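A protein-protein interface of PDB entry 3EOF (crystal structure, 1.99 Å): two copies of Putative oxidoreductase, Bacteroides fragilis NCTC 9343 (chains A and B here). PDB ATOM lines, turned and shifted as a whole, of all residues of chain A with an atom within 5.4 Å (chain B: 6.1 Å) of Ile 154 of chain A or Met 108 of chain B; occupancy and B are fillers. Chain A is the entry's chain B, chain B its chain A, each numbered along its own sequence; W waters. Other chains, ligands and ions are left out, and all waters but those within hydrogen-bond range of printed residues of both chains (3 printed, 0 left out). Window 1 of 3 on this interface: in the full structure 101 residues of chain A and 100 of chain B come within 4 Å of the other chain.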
ATOM      1  N   PHE A  77      -8.208 -31.072  -0.540  1.00  0.00           N
ATOM      2  CA  PHE A  77      -8.209 -31.457  -1.937  1.00  0.00           C
ATOM      3  C   PHE A  77      -7.175 -32.558  -2.039  1.00  0.00           C
ATOM      4  O   PHE A  77      -6.016 -32.368  -1.707  1.00  0.00           O
ATOM      5  CB  PHE A  77      -7.828 -30.265  -2.836  1.00  0.00           C
ATOM      6  CG  PHE A  77      -8.865 -29.147  -2.833  1.00  0.00           C
ATOM      7  CD1 PHE A  77      -8.834 -28.163  -1.886  1.00  0.00           C
ATOM      8  CD2 PHE A  77      -9.898 -29.168  -3.762  1.00  0.00           C
ATOM      9  CE1 PHE A  77      -9.778 -27.159  -1.935  1.00  0.00           C
ATOM     10  CE2 PHE A  77     -10.846 -28.204  -3.797  1.00  0.00           C
ATOM     11  CZ  PHE A  77     -10.801 -27.212  -2.882  1.00  0.00           C
ATOM     12  N   CYS A  78      -7.605 -33.700  -2.529  1.00  0.00           N
ATOM     13  CA  CYS A  78      -6.770 -34.884  -2.568  1.00  0.00           C
ATOM     14  C   CYS A  78      -6.551 -35.409  -3.964  1.00  0.00           C
ATOM     15  O   CYS A  78      -7.464 -35.472  -4.743  1.00  0.00           O
ATOM     16  CB  CYS A  78      -7.465 -35.990  -1.767  1.00  0.00           C
ATOM     17  SG  CYS A  78      -7.735 -35.649  -0.046  1.00  0.00           S
ATOM     18  N   ALA A  79      -5.314 -35.755  -4.268  1.00  0.00           N
ATOM     19  CA  ALA A  79      -5.002 -36.495  -5.479  1.00  0.00           C
ATOM     20  C   ALA A  79      -5.729 -37.818  -5.280  1.00  0.00           C
ATOM     21  O   ALA A  79      -5.684 -38.403  -4.212  1.00  0.00           O
ATOM     22  CB  ALA A  79      -3.528 -36.724  -5.589  1.00  0.00           C
ATOM     23  N   PHE A 103       0.859 -39.976  -9.476  1.00  0.00           N
ATOM     24  CA  PHE A 103       0.695 -39.069  -8.369  1.00  0.00           C
ATOM     25  C   PHE A 103       0.739 -37.640  -8.869  1.00  0.00           C
ATOM     26  O   PHE A 103      -0.132 -36.855  -8.548  1.00  0.00           O
ATOM     27  CB  PHE A 103       1.782 -39.269  -7.275  1.00  0.00           C
ATOM     28  CG  PHE A 103       1.742 -38.188  -6.237  1.00  0.00           C
ATOM     29  CD1 PHE A 103       0.673 -38.098  -5.354  1.00  0.00           C
ATOM     30  CD2 PHE A 103       2.714 -37.203  -6.212  1.00  0.00           C
ATOM     31  CE1 PHE A 103       0.615 -37.068  -4.424  1.00  0.00           C
ATOM     32  CE2 PHE A 103       2.648 -36.191  -5.307  1.00  0.00           C
ATOM     33  CZ  PHE A 103       1.599 -36.111  -4.410  1.00  0.00           C
ATOM     34  N   ALA A 107      -2.089 -34.913  -8.813  1.00  0.00           N
ATOM     35  CA  ALA A 107      -1.790 -33.699  -8.041  1.00  0.00           C
ATOM     36  C   ALA A 107      -2.084 -32.440  -8.853  1.00  0.00           C
ATOM     37  O   ALA A 107      -2.696 -31.517  -8.375  1.00  0.00           O
ATOM     38  CB  ALA A 107      -0.297 -33.732  -7.545  1.00  0.00           C
ATOM     39  N   THR A 110      -5.695 -32.018  -9.190  1.00  0.00           N
ATOM     40  CA  THR A 110      -6.203 -31.538  -7.910  1.00  0.00           C
ATOM     41  C   THR A 110      -5.980 -30.061  -7.679  1.00  0.00           C
ATOM     42  O   THR A 110      -6.899 -29.345  -7.239  1.00  0.00           O
ATOM     43  CB  THR A 110      -5.618 -32.419  -6.740  1.00  0.00           C
ATOM     44  OG1 THR A 110      -5.912 -33.798  -7.029  1.00  0.00           O
ATOM     45  CG2 THR A 110      -6.198 -32.024  -5.357  1.00  0.00           C
ATOM     46  N   LEU A 111      -4.771 -29.591  -7.979  1.00  0.00           N
ATOM     47  CA  LEU A 111      -4.434 -28.170  -7.805  1.00  0.00           C
ATOM     48  C   LEU A 111      -5.252 -27.224  -8.685  1.00  0.00           C
ATOM     49  O   LEU A 111      -5.699 -26.128  -8.247  1.00  0.00           O
ATOM     50  CB  LEU A 111      -2.935 -27.994  -7.960  1.00  0.00           C
ATOM     51  CG  LEU A 111      -2.158 -28.638  -6.800  1.00  0.00           C
ATOM     52  CD1 LEU A 111      -0.748 -29.106  -7.178  1.00  0.00           C
ATOM     53  CD2 LEU A 111      -2.094 -27.698  -5.639  1.00  0.00           C
ATOM     54  N   THR A 134      -0.313 -29.126   4.644  1.00  0.00           N
ATOM     55  CA  THR A 134      -0.899 -30.338   4.110  1.00  0.00           C
ATOM     56  C   THR A 134       0.170 -31.379   3.762  1.00  0.00           C
ATOM     57  O   THR A 134       0.051 -32.537   4.125  1.00  0.00           O
ATOM     58  CB  THR A 134      -1.830 -30.065   2.871  1.00  0.00           C
ATOM     59  OG1 THR A 134      -2.934 -29.260   3.271  1.00  0.00           O
ATOM     60  CG2 THR A 134      -2.385 -31.346   2.335  1.00  0.00           C
ATOM     61  N   THR A 135       1.231 -30.927   3.108  1.00  0.00           N
ATOM     62  CA  THR A 135       2.335 -31.793   2.711  1.00  0.00           C
ATOM     63  C   THR A 135       3.462 -31.883   3.761  1.00  0.00           C
ATOM     64  O   THR A 135       4.461 -32.538   3.509  1.00  0.00           O
ATOM     65  CB  THR A 135       2.852 -31.403   1.315  1.00  0.00           C
ATOM     66  OG1 THR A 135       3.027 -29.992   1.261  1.00  0.00           O
ATOM     67  CG2 THR A 135       1.801 -31.788   0.250  1.00  0.00           C
ATOM     68  N   PHE A 152      -4.175 -39.077  -1.757  1.00  0.00           N
ATOM     69  CA  PHE A 152      -3.121 -38.320  -1.086  1.00  0.00           C
ATOM     70  C   PHE A 152      -3.560 -36.877  -0.973  1.00  0.00           C
ATOM     71  O   PHE A 152      -3.994 -36.301  -1.966  1.00  0.00           O
ATOM     72  CB  PHE A 152      -1.816 -38.445  -1.892  1.00  0.00           C
ATOM     73  CG  PHE A 152      -0.586 -38.019  -1.149  1.00  0.00           C
ATOM     74  CD1 PHE A 152      -0.287 -36.683  -1.013  1.00  0.00           C
ATOM     75  CD2 PHE A 152       0.276 -38.960  -0.584  1.00  0.00           C
ATOM     76  CE1 PHE A 152       0.834 -36.260  -0.325  1.00  0.00           C
ATOM     77  CE2 PHE A 152       1.401 -38.557   0.090  1.00  0.00           C
ATOM     78  CZ  PHE A 152       1.683 -37.199   0.237  1.00  0.00           C
ATOM     79  N   PRO A 153      -3.437 -36.279   0.231  1.00  0.00           N
ATOM     80  CA  PRO A 153      -3.879 -34.895   0.385  1.00  0.00           C
ATOM     81  C   PRO A 153      -2.818 -33.984  -0.223  1.00  0.00           C
ATOM     82  O   PRO A 153      -1.638 -34.139   0.061  1.00  0.00           O
ATOM     83  CB  PRO A 153      -3.993 -34.721   1.901  1.00  0.00           C
ATOM     84  CG  PRO A 153      -2.940 -35.648   2.474  1.00  0.00           C
ATOM     85  CD  PRO A 153      -2.881 -36.825   1.488  1.00  0.00           C
ATOM     86  N   ILE A 154      -3.246 -33.080  -1.089  1.00  0.00           N
ATOM     87  CA  ILE A 154      -2.328 -32.207  -1.825  1.00  0.00           C
ATOM     88  C   ILE A 154      -2.356 -30.857  -1.178  1.00  0.00           C
ATOM     89  O   ILE A 154      -1.320 -30.262  -0.891  1.00  0.00           O
ATOM     90  CB  ILE A 154      -2.696 -32.105  -3.332  1.00  0.00           C
ATOM     91  CG1 ILE A 154      -2.623 -33.493  -3.956  1.00  0.00           C
ATOM     92  CG2 ILE A 154      -1.727 -31.109  -4.083  1.00  0.00           C
ATOM     93  CD1 ILE A 154      -1.203 -34.062  -3.921  1.00  0.00           C
ATOM     94  N   THR A 155      -3.538 -30.351  -0.972  1.00  0.00           N
ATOM     95  CA  THR A 155      -3.645 -29.066  -0.310  1.00  0.00           C
ATOM     96  C   THR A 155      -4.983 -29.011   0.397  1.00  0.00           C
ATOM     97  O   THR A 155      -5.864 -29.846   0.147  1.00  0.00           O
ATOM     98  CB  THR A 155      -3.356 -27.855  -1.288  1.00  0.00           C
ATOM     99  OG1 THR A 155      -3.291 -26.612  -0.546  1.00  0.00           O
ATOM    100  CG2 THR A 155      -4.389 -27.788  -2.388  1.00  0.00           C
ATOM    101  N   THR A 156      -5.049 -28.047   1.321  1.00  0.00           N
ATOM    102  CA  THR A 156      -6.164 -27.773   2.201  1.00  0.00           C
ATOM    103  C   THR A 156      -6.479 -26.300   2.142  1.00  0.00           C
ATOM    104  O   THR A 156      -5.582 -25.454   2.188  1.00  0.00           O
ATOM    105  CB  THR A 156      -5.851 -28.116   3.651  1.00  0.00           C
ATOM    106  OG1 THR A 156      -5.492 -29.491   3.728  1.00  0.00           O
ATOM    107  CG2 THR A 156      -7.050 -27.879   4.553  1.00  0.00           C
ATOM    108  N   SER B  36      -2.317 -17.373  -4.885  1.00  0.00           N
ATOM    109  CA  SER B  36      -1.643 -17.626  -3.621  1.00  0.00           C
ATOM    110  C   SER B  36      -0.336 -18.219  -3.940  1.00  0.00           C
ATOM    111  O   SER B  36      -0.213 -18.975  -4.930  1.00  0.00           O
ATOM    112  CB  SER B  36      -2.441 -18.583  -2.767  1.00  0.00           C
ATOM    113  OG  SER B  36      -3.653 -17.988  -2.439  1.00  0.00           O
ATOM    114  N   MET B  38       3.358 -19.676  -1.776  1.00  0.00           N
ATOM    115  CA  MET B  38       3.964 -20.039  -0.496  1.00  0.00           C
ATOM    116  C   MET B  38       4.948 -19.012  -0.078  1.00  0.00           C
ATOM    117  O   MET B  38       5.909 -18.732  -0.816  1.00  0.00           O
ATOM    118  CB  MET B  38       4.704 -21.357  -0.592  1.00  0.00           C
ATOM    119  CG  MET B  38       5.209 -21.833   0.742  1.00  0.00           C
ATOM    120  SD  MET B  38       6.235 -23.489   0.435  1.00  0.00           S
ATOM    121  CE  MET B  38       7.996 -22.697   0.413  1.00  0.00           C
ATOM    122  N   MET B 101      10.650 -31.873  -1.620  1.00  0.00           N
ATOM    123  CA  MET B 101       9.641 -31.085  -0.928  1.00  0.00           C
ATOM    124  C   MET B 101       9.504 -29.724  -1.543  1.00  0.00           C
ATOM    125  O   MET B 101       8.397 -29.263  -1.776  1.00  0.00           O
ATOM    126  CB  MET B 101      10.013 -30.903   0.533  1.00  0.00           C
ATOM    127  CG  MET B 101       8.987 -30.113   1.351  1.00  0.00           C
ATOM    128  SD  MET B 101       7.179 -31.037   1.511  1.00  0.00           S
ATOM    129  CE  MET B 101       6.422 -29.731   2.808  1.00  0.00           C
ATOM    130  N   PHE B 103      10.586 -28.830  -4.514  1.00  0.00           N
ATOM    131  CA  PHE B 103      10.071 -28.996  -5.868  1.00  0.00           C
ATOM    132  C   PHE B 103       8.563 -29.070  -5.876  1.00  0.00           C
ATOM    133  O   PHE B 103       7.898 -28.427  -6.685  1.00  0.00           O
ATOM    134  CB  PHE B 103      10.636 -30.274  -6.577  1.00  0.00           C
ATOM    135  CG  PHE B 103       9.832 -30.667  -7.794  1.00  0.00           C
ATOM    136  CD1 PHE B 103       9.913 -29.920  -8.973  1.00  0.00           C
ATOM    137  CD2 PHE B 103       8.883 -31.697  -7.714  1.00  0.00           C
ATOM    138  CE1 PHE B 103       9.107 -30.226 -10.082  1.00  0.00           C
ATOM    139  CE2 PHE B 103       8.098 -32.024  -8.824  1.00  0.00           C
ATOM    140  CZ  PHE B 103       8.210 -31.285 -10.007  1.00  0.00           C
ATOM    141  N   LEU B 104       7.994 -29.848  -4.974  1.00  0.00           N
ATOM    142  CA  LEU B 104       6.549 -29.932  -4.897  1.00  0.00           C
ATOM    143  C   LEU B 104       5.931 -28.596  -4.483  1.00  0.00           C
ATOM    144  O   LEU B 104       4.883 -28.217  -4.995  1.00  0.00           O
ATOM    145  CB  LEU B 104       6.099 -31.052  -3.965  1.00  0.00           C
ATOM    146  CG  LEU B 104       4.581 -31.219  -3.819  1.00  0.00           C
ATOM    147  CD1 LEU B 104       3.892 -31.493  -5.139  1.00  0.00           C
ATOM    148  CD2 LEU B 104       4.266 -32.319  -2.747  1.00  0.00           C
ATOM    149  N   ASN B 105       6.555 -27.892  -3.561  1.00  0.00           N
ATOM    150  CA  ASN B 105       6.057 -26.576  -3.166  1.00  0.00           C
ATOM    151  C   ASN B 105       6.048 -25.606  -4.336  1.00  0.00           C
ATOM    152  O   ASN B 105       5.097 -24.858  -4.493  1.00  0.00           O
ATOM    153  CB  ASN B 105       6.909 -25.942  -2.034  1.00  0.00           C
ATOM    154  CG  ASN B 105       6.715 -26.611  -0.668  1.00  0.00           C
ATOM    155  OD1 ASN B 105       5.648 -27.146  -0.401  1.00  0.00           O
ATOM    156  ND2 ASN B 105       7.785 -26.575   0.212  1.00  0.00           N
ATOM    157  N   ALA B 106       7.100 -25.634  -5.173  1.00  0.00           N
ATOM    158  CA  ALA B 106       7.221 -24.727  -6.318  1.00  0.00           C
ATOM    159  C   ALA B 106       6.184 -25.112  -7.353  1.00  0.00           C
ATOM    160  O   ALA B 106       5.538 -24.232  -7.923  1.00  0.00           O
ATOM    161  CB  ALA B 106       8.621 -24.750  -6.926  1.00  0.00           C
ATOM    162  N   ALA B 107       6.048 -26.429  -7.593  1.00  0.00           N
ATOM    163  CA  ALA B 107       5.061 -26.992  -8.526  1.00  0.00           C
ATOM    164  C   ALA B 107       3.662 -26.489  -8.201  1.00  0.00           C
ATOM    165  O   ALA B 107       2.893 -26.112  -9.085  1.00  0.00           O
ATOM    166  CB  ALA B 107       5.070 -28.471  -8.468  1.00  0.00           C
ATOM    167  N   MET B 108       3.320 -26.560  -6.943  1.00  0.00           N
ATOM    168  CA  MET B 108       2.021 -26.079  -6.511  1.00  0.00           C
ATOM    169  C   MET B 108       1.868 -24.634  -6.775  1.00  0.00           C
ATOM    170  O   MET B 108       0.782 -24.206  -7.159  1.00  0.00           O
ATOM    171  CB  MET B 108       1.773 -26.355  -5.044  1.00  0.00           C
ATOM    172  CG  MET B 108       1.694 -27.858  -4.765  1.00  0.00           C
ATOM    173  SD  MET B 108       1.069 -28.312  -2.936  1.00  0.00           S
ATOM    174  CE  MET B 108       2.557 -27.649  -1.890  1.00  0.00           C
ATOM    175  N   ASP B 109       2.907 -23.854  -6.511  1.00  0.00           N
ATOM    176  CA  ASP B 109       2.819 -22.399  -6.746  1.00  0.00           C
ATOM    177  C   ASP B 109       2.522 -22.168  -8.203  1.00  0.00           C
ATOM    178  O   ASP B 109       1.719 -21.346  -8.581  1.00  0.00           O
ATOM    179  CB  ASP B 109       4.131 -21.670  -6.388  1.00  0.00           C
ATOM    180  CG  ASP B 109       4.078 -20.887  -5.066  1.00  0.00           C
ATOM    181  OD1 ASP B 109       3.308 -21.256  -4.129  1.00  0.00           O
ATOM    182  OD2 ASP B 109       4.885 -19.888  -4.980  1.00  0.00           O
ATOM    183  N   THR B 110       3.193 -22.955  -9.018  1.00  0.00           N
ATOM    184  CA  THR B 110       3.142 -22.850 -10.456  1.00  0.00           C
ATOM    185  C   THR B 110       1.816 -23.248 -11.071  1.00  0.00           C
ATOM    186  O   THR B 110       1.423 -22.683 -12.087  1.00  0.00           O
ATOM    187  CB  THR B 110       4.264 -23.730 -11.062  1.00  0.00           C
ATOM    188  OG1 THR B 110       5.512 -23.374 -10.459  1.00  0.00           O
ATOM    189  CG2 THR B 110       4.379 -23.567 -12.555  1.00  0.00           C
ATOM    190  N   LEU B 111       1.191 -24.271 -10.505  1.00  0.00           N
ATOM    191  CA  LEU B 111      -0.062 -24.789 -11.004  1.00  0.00           C
ATOM    192  C   LEU B 111      -1.183 -23.824 -10.636  1.00  0.00           C
ATOM    193  O   LEU B 111      -2.116 -23.662 -11.401  1.00  0.00           O
ATOM    194  CB  LEU B 111      -0.332 -26.175 -10.481  1.00  0.00           C
ATOM    195  CG  LEU B 111       0.571 -27.201 -11.189  1.00  0.00           C
ATOM    196  CD1 LEU B 111       0.665 -28.470 -10.362  1.00  0.00           C
ATOM    197  CD2 LEU B 111       0.018 -27.449 -12.532  1.00  0.00           C
ATOM    198  N   LEU B 112      -1.057 -23.187  -9.483  1.00  0.00           N
ATOM    199  CA  LEU B 112      -2.046 -22.155  -9.050  1.00  0.00           C
ATOM    200  C   LEU B 112      -2.070 -20.973  -9.987  1.00  0.00           C
ATOM    201  O   LEU B 112      -3.124 -20.475 -10.343  1.00  0.00           O
ATOM    202  CB  LEU B 112      -1.724 -21.713  -7.635  1.00  0.00           C
ATOM    203  CG  LEU B 112      -2.389 -22.467  -6.489  1.00  0.00           C
ATOM    204  CD1 LEU B 112      -2.621 -23.953  -6.639  1.00  0.00           C
ATOM    205  CD2 LEU B 112      -1.614 -22.179  -5.243  1.00  0.00           C
ATOM    206  N   VAL B 113      -0.883 -20.502 -10.371  1.00  0.00           N
ATOM    207  CA  VAL B 113      -0.765 -19.445 -11.381  1.00  0.00           C
ATOM    208  C   VAL B 113      -1.344 -19.876 -12.733  1.00  0.00           C
ATOM    209  O   VAL B 113      -2.126 -19.153 -13.353  1.00  0.00           O
ATOM    210  CB  VAL B 113       0.728 -19.000 -11.587  1.00  0.00           C
ATOM    211  CG1 VAL B 113       0.876 -18.160 -12.799  1.00  0.00           C
ATOM    212  CG2 VAL B 113       1.239 -18.286 -10.385  1.00  0.00           C
HETATM  213  O   HOH W   1       4.037 -26.731   1.666  1.00  0.00           O
HETATM  214  O   HOH W   2       0.148 -28.127   0.440  1.00  0.00           O
HETATM  215  O   HOH W   3       5.127 -29.764  -0.612  1.00  0.00           O
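The side-chain amide nitrogen (ND2) of Asn 105 of chain B sits close to the backbone carbonyl oxygen (O) of Met 101 of chain B, 3.4 Å away. O of Phe 77 of chain A is in hydrogen-bond range of N of Ile 154 of chain A (2.9 Å).
O of Thr 135 of chain A lies close to SD of Met 101 of chain B (3.7 Å). The side-chain sulfur (SD) of Met 108 of chain B lies close to the backbone carbonyl oxygen (O) of Ile 154 of chain A (3.7 Å).
Among the printed residues, merely in contact across the chains: Leu 111 of chain A with Met 108 of chain B (3.7 Å), Leu 111 of chain A with Leu 111 of chain B (3.5 Å), Leu 111 of chain A with Leu 112 of chain B (3.9 Å), Thr 135 of chain A with Leu 104 of chain B (3.9 Å) and Thr 135 of chain A with Met 108 of chain B (3.95 Å).
Of the 14 printed residues of chain A, 3 touch a printed residue of chain B. Hydrophobic or aromatic side chains of chain A within 4 Å of the printed part of chain B: Leu 111. Along chain A the printed residues that touch a printed residue of chain B span positions 111 to 154. Among the printed residues, no Asp or Glu carboxylate lies within 4 Å of a Lys or Arg side-chain nitrogen of the other chain.
Phe 103 of chain A touches none of the printed residues of chain B. Of the printed residues of chain B, Leu 111 of chain A touches Met 108, Leu 111 and Leu 112. Printed residues of chain B within 4 Å of Thr 135 of chain A: Met 101 (3.5 Å), Leu 104 (3.9 Å) and Met 108 (3.95 Å). Of chain B, only Met 108 comes within 4 Å of Ile 154 of chain A. Of the printed residues of chain A, Met 101 of chain B touches Thr 135 (3.5 Å). Of the printed residues of chain A, Leu 104 of chain B touches Thr 135 (3.9 Å). Printed residues of chain A within 4 Å of Met 108 of chain B: Leu 111 (3.7 Å), Thr 135 (3.95 Å) and Ile 154 (3.7 Å). The nearest residue of chain B that does not touch Ile 154 of chain A is Leu 104 of chain B (5.7 Å). The nearest residue of chain A that does not touch Met 108 of chain B is Thr 155 of chain A (4.7 Å). The nearest printed residue of chain B that does not touch Thr 135 of chain A is Asn 105 of chain B (4.2 Å).
Leu 111 of chain A touches its own counterpart, Leu 111 of chain B. Positions printed for both chains: 103, 107, 110 and 111. Of the 7 pairs that touch across the chains among the printed residues, 1 has its exchanged pair printed and touching as well.
Water W1 bridges OD1 of Asn 105 of chain B (2.7 Å) and OG1 of Thr 135 of chain A (3.4 Å). Water W3 lies within hydrogen-bond range of the side-chain amide oxygen (OD1) of Asn 105 of chain B (2.7 Å), the side-chain hydroxyl (OG1) of Thr 135 of chain A (2.8 Å) and the side-chain sulfur (SD) of Met 101 of chain B (3.2 Å). Water W2 bridges the backbone carbonyl oxygen of Ile 154 of chain A and the side-chain sulfur of Met 108 of chain B.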
